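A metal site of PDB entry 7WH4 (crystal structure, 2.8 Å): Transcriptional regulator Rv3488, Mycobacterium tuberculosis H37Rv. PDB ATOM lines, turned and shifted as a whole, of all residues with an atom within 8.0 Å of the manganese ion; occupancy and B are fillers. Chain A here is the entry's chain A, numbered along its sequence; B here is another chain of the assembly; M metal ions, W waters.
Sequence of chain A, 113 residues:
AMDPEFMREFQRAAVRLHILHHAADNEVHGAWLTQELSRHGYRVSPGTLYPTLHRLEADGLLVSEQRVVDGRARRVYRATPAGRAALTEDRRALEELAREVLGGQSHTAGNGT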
ATOM      1  N   HIS A  18     -29.111  30.555   2.697  1.00  0.00           N
ATOM      2  CA  HIS A  18     -28.326  30.110   3.849  1.00  0.00           C
ATOM      3  C   HIS A  18     -27.611  31.290   4.495  1.00  0.00           C
ATOM      4  O   HIS A  18     -27.522  31.363   5.728  1.00  0.00           O
ATOM      5  CB  HIS A  18     -27.371  28.980   3.459  1.00  0.00           C
ATOM      6  CG  HIS A  18     -27.961  27.625   3.671  1.00  0.00           C
ATOM      7  ND1 HIS A  18     -28.121  27.087   4.937  1.00  0.00           N
ATOM      8  CD2 HIS A  18     -28.466  26.722   2.805  1.00  0.00           C
ATOM      9  CE1 HIS A  18     -28.691  25.902   4.832  1.00  0.00           C
ATOM     10  NE2 HIS A  18     -28.903  25.660   3.538  1.00  0.00           N
ATOM     11  N   HIS A  21     -30.132  33.259   6.385  1.00  0.00           N
ATOM     12  CA  HIS A  21     -30.500  32.479   7.546  1.00  0.00           C
ATOM     13  C   HIS A  21     -29.476  32.673   8.658  1.00  0.00           C
ATOM     14  O   HIS A  21     -29.839  32.967   9.805  1.00  0.00           O
ATOM     15  CB  HIS A  21     -30.709  31.006   7.164  1.00  0.00           C
ATOM     16  CG  HIS A  21     -30.888  30.089   8.321  1.00  0.00           C
ATOM     17  ND1 HIS A  21     -29.934  29.134   8.639  1.00  0.00           N
ATOM     18  CD2 HIS A  21     -31.879  29.958   9.225  1.00  0.00           C
ATOM     19  CE1 HIS A  21     -30.345  28.457   9.694  1.00  0.00           C
ATOM     20  NE2 HIS A  21     -31.532  28.953  10.075  1.00  0.00           N
ATOM     21  N   HIS A  22     -28.182  32.544   8.296  1.00  0.00           N
ATOM     22  CA  HIS A  22     -27.093  32.636   9.247  1.00  0.00           C
ATOM     23  C   HIS A  22     -26.915  34.076   9.727  1.00  0.00           C
ATOM     24  O   HIS A  22     -26.701  34.319  10.921  1.00  0.00           O
ATOM     25  CB  HIS A  22     -25.810  32.035   8.641  1.00  0.00           C
ATOM     26  CG  HIS A  22     -25.774  30.540   8.660  1.00  0.00           C
ATOM     27  ND1 HIS A  22     -26.484  29.774   7.755  1.00  0.00           N
ATOM     28  CD2 HIS A  22     -25.119  29.687   9.474  1.00  0.00           C
ATOM     29  CE1 HIS A  22     -26.266  28.492   8.013  1.00  0.00           C
ATOM     30  NE2 HIS A  22     -25.423  28.415   9.056  1.00  0.00           N
ATOM     31  N   ASP A  25     -29.550  35.180  12.252  1.00  0.00           N
ATOM     32  CA  ASP A  25     -29.376  34.667  13.604  1.00  0.00           C
ATOM     33  C   ASP A  25     -28.350  35.517  14.367  1.00  0.00           C
ATOM     34  O   ASP A  25     -28.512  35.743  15.560  1.00  0.00           O
ATOM     35  CB  ASP A  25     -29.069  33.165  13.607  1.00  0.00           C
ATOM     36  CG  ASP A  25     -30.278  32.290  13.292  1.00  0.00           C
ATOM     37  OD1 ASP A  25     -31.410  32.808  13.272  1.00  0.00           O
ATOM     38  OD2 ASP A  25     -30.073  31.081  13.077  1.00  0.00           O
ATOM     39  N   TRP A  32     -16.348  32.520   8.267  1.00  0.00           N
ATOM     40  CA  TRP A  32     -17.240  31.655   9.013  1.00  0.00           C
ATOM     41  C   TRP A  32     -18.410  31.191   8.150  1.00  0.00           C
ATOM     42  O   TRP A  32     -18.840  30.031   8.253  1.00  0.00           O
ATOM     43  CB  TRP A  32     -17.744  32.362  10.266  1.00  0.00           C
ATOM     44  CG  TRP A  32     -18.450  31.431  11.206  1.00  0.00           C
ATOM     45  CD1 TRP A  32     -17.876  30.509  12.026  1.00  0.00           C
ATOM     46  CD2 TRP A  32     -19.865  31.355  11.444  1.00  0.00           C
ATOM     47  NE1 TRP A  32     -18.829  29.857  12.758  1.00  0.00           N
ATOM     48  CE2 TRP A  32     -20.058  30.341  12.417  1.00  0.00           C
ATOM     49  CE3 TRP A  32     -20.979  32.015  10.930  1.00  0.00           C
ATOM     50  CZ2 TRP A  32     -21.325  29.992  12.882  1.00  0.00           C
ATOM     51  CZ3 TRP A  32     -22.240  31.669  11.388  1.00  0.00           C
ATOM     52  CH2 TRP A  32     -22.404  30.664  12.361  1.00  0.00           C
ATOM     53  N   GLN A  35     -17.386  28.259   6.094  1.00  0.00           N
ATOM     54  CA  GLN A  35     -17.311  27.016   6.830  1.00  0.00           C
ATOM     55  C   GLN A  35     -18.708  26.465   7.108  1.00  0.00           C
ATOM     56  O   GLN A  35     -18.949  25.264   6.946  1.00  0.00           O
ATOM     57  CB  GLN A  35     -16.493  27.191   8.115  1.00  0.00           C
ATOM     58  N   GLU A  36     -19.631  27.362   7.490  1.00  0.00           N
ATOM     59  CA  GLU A  36     -20.988  26.961   7.819  1.00  0.00           C
ATOM     60  C   GLU A  36     -21.701  26.410   6.591  1.00  0.00           C
ATOM     61  O   GLU A  36     -22.447  25.420   6.695  1.00  0.00           O
ATOM     62  CB  GLU A  36     -21.780  28.121   8.425  1.00  0.00           C
ATOM     63  CG  GLU A  36     -21.749  28.155   9.947  1.00  0.00           C
ATOM     64  CD  GLU A  36     -22.038  26.854  10.682  1.00  0.00           C
ATOM     65  OE1 GLU A  36     -21.128  26.371  11.370  1.00  0.00           O
ATOM     66  OE2 GLU A  36     -23.173  26.336  10.569  1.00  0.00           O
ATOM     67  N   LEU A  37     -21.444  27.027   5.426  1.00  0.00           N
ATOM     68  CA  LEU A  37     -22.039  26.655   4.145  1.00  0.00           C
ATOM     69  C   LEU A  37     -21.542  25.268   3.715  1.00  0.00           C
ATOM     70  O   LEU A  37     -22.337  24.447   3.254  1.00  0.00           O
ATOM     71  CB  LEU A  37     -21.688  27.716   3.091  1.00  0.00           C
ATOM     72  CG  LEU A  37     -22.518  29.002   3.104  1.00  0.00           C
ATOM     73  CD1 LEU A  37     -21.831  30.091   2.298  1.00  0.00           C
ATOM     74  CD2 LEU A  37     -23.918  28.759   2.577  1.00  0.00           C
ATOM     75  N   ARG A  39     -20.430  22.953   5.696  1.00  0.00           N
ATOM     76  CA  ARG A  39     -21.032  22.034   6.646  1.00  0.00           C
ATOM     77  C   ARG A  39     -22.424  21.614   6.182  1.00  0.00           C
ATOM     78  O   ARG A  39     -22.845  20.486   6.427  1.00  0.00           O
ATOM     79  CB  ARG A  39     -21.021  22.649   8.058  1.00  0.00           C
ATOM     80  CG  ARG A  39     -22.081  22.094   9.001  1.00  0.00           C
ATOM     81  CD  ARG A  39     -22.301  22.936  10.247  1.00  0.00           C
ATOM     82  NE  ARG A  39     -21.067  23.151  11.017  1.00  0.00           N
ATOM     83  N   HIS A  40     -23.110  22.533   5.481  1.00  0.00           N
ATOM     84  CA  HIS A  40     -24.471  22.293   5.004  1.00  0.00           C
ATOM     85  C   HIS A  40     -24.459  21.682   3.600  1.00  0.00           C
ATOM     86  O   HIS A  40     -25.523  21.440   3.017  1.00  0.00           O
ATOM     87  CB  HIS A  40     -25.332  23.558   5.121  1.00  0.00           C
ATOM     88  CG  HIS A  40     -25.699  23.924   6.524  1.00  0.00           C
ATOM     89  ND1 HIS A  40     -26.736  23.322   7.212  1.00  0.00           N
ATOM     90  CD2 HIS A  40     -25.181  24.848   7.354  1.00  0.00           C
ATOM     91  CE1 HIS A  40     -26.837  23.845   8.415  1.00  0.00           C
ATOM     92  NE2 HIS A  40     -25.900  24.798   8.527  1.00  0.00           N
ATOM     93  N   GLU B 100     -34.208  23.496   6.133  1.00  0.00           N
ATOM     94  CA  GLU B 100     -32.832  23.818   6.497  1.00  0.00           C
ATOM     95  C   GLU B 100     -32.773  25.213   7.123  1.00  0.00           C
ATOM     96  O   GLU B 100     -32.070  25.403   8.115  1.00  0.00           O
ATOM     97  CB  GLU B 100     -31.957  23.756   5.249  1.00  0.00           C
ATOM     98  CG  GLU B 100     -30.640  23.003   5.435  1.00  0.00           C
ATOM     99  CD  GLU B 100     -30.131  22.238   4.210  1.00  0.00           C
ATOM    100  OE1 GLU B 100     -29.137  22.689   3.598  1.00  0.00           O
ATOM    101  OE2 GLU B 100     -30.719  21.185   3.894  1.00  0.00           O
HETATM  102 MN    MN M   1     -25.475  26.302  10.703  1.00  0.00          MN
HETATM  103  O   HOH W   1     -28.125  25.841  10.445  1.00  0.00           O
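The manganese ion is bound by the side-chain carboxylate of Glu 36 (2.3 Å), a ring nitrogen (NE2) of His 40 (2.7 Å), a ring nitrogen (NE2) of His 22 (2.7 Å) and water W1 (2.7 Å). The manganese ion has four donor atoms within binding distance.
Within 4 Å of the manganese ion: His 22, Glu 36 and His 40.
The side-chain carboxylate of Glu 36 lies within salt-bridge range of the guanidinium group of Arg 39 (3.2 Å). A ring nitrogen (ND1) of His 22 is in hydrogen-bond range of the backbone carbonyl oxygen (O) of His 18 (2.8 Å).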
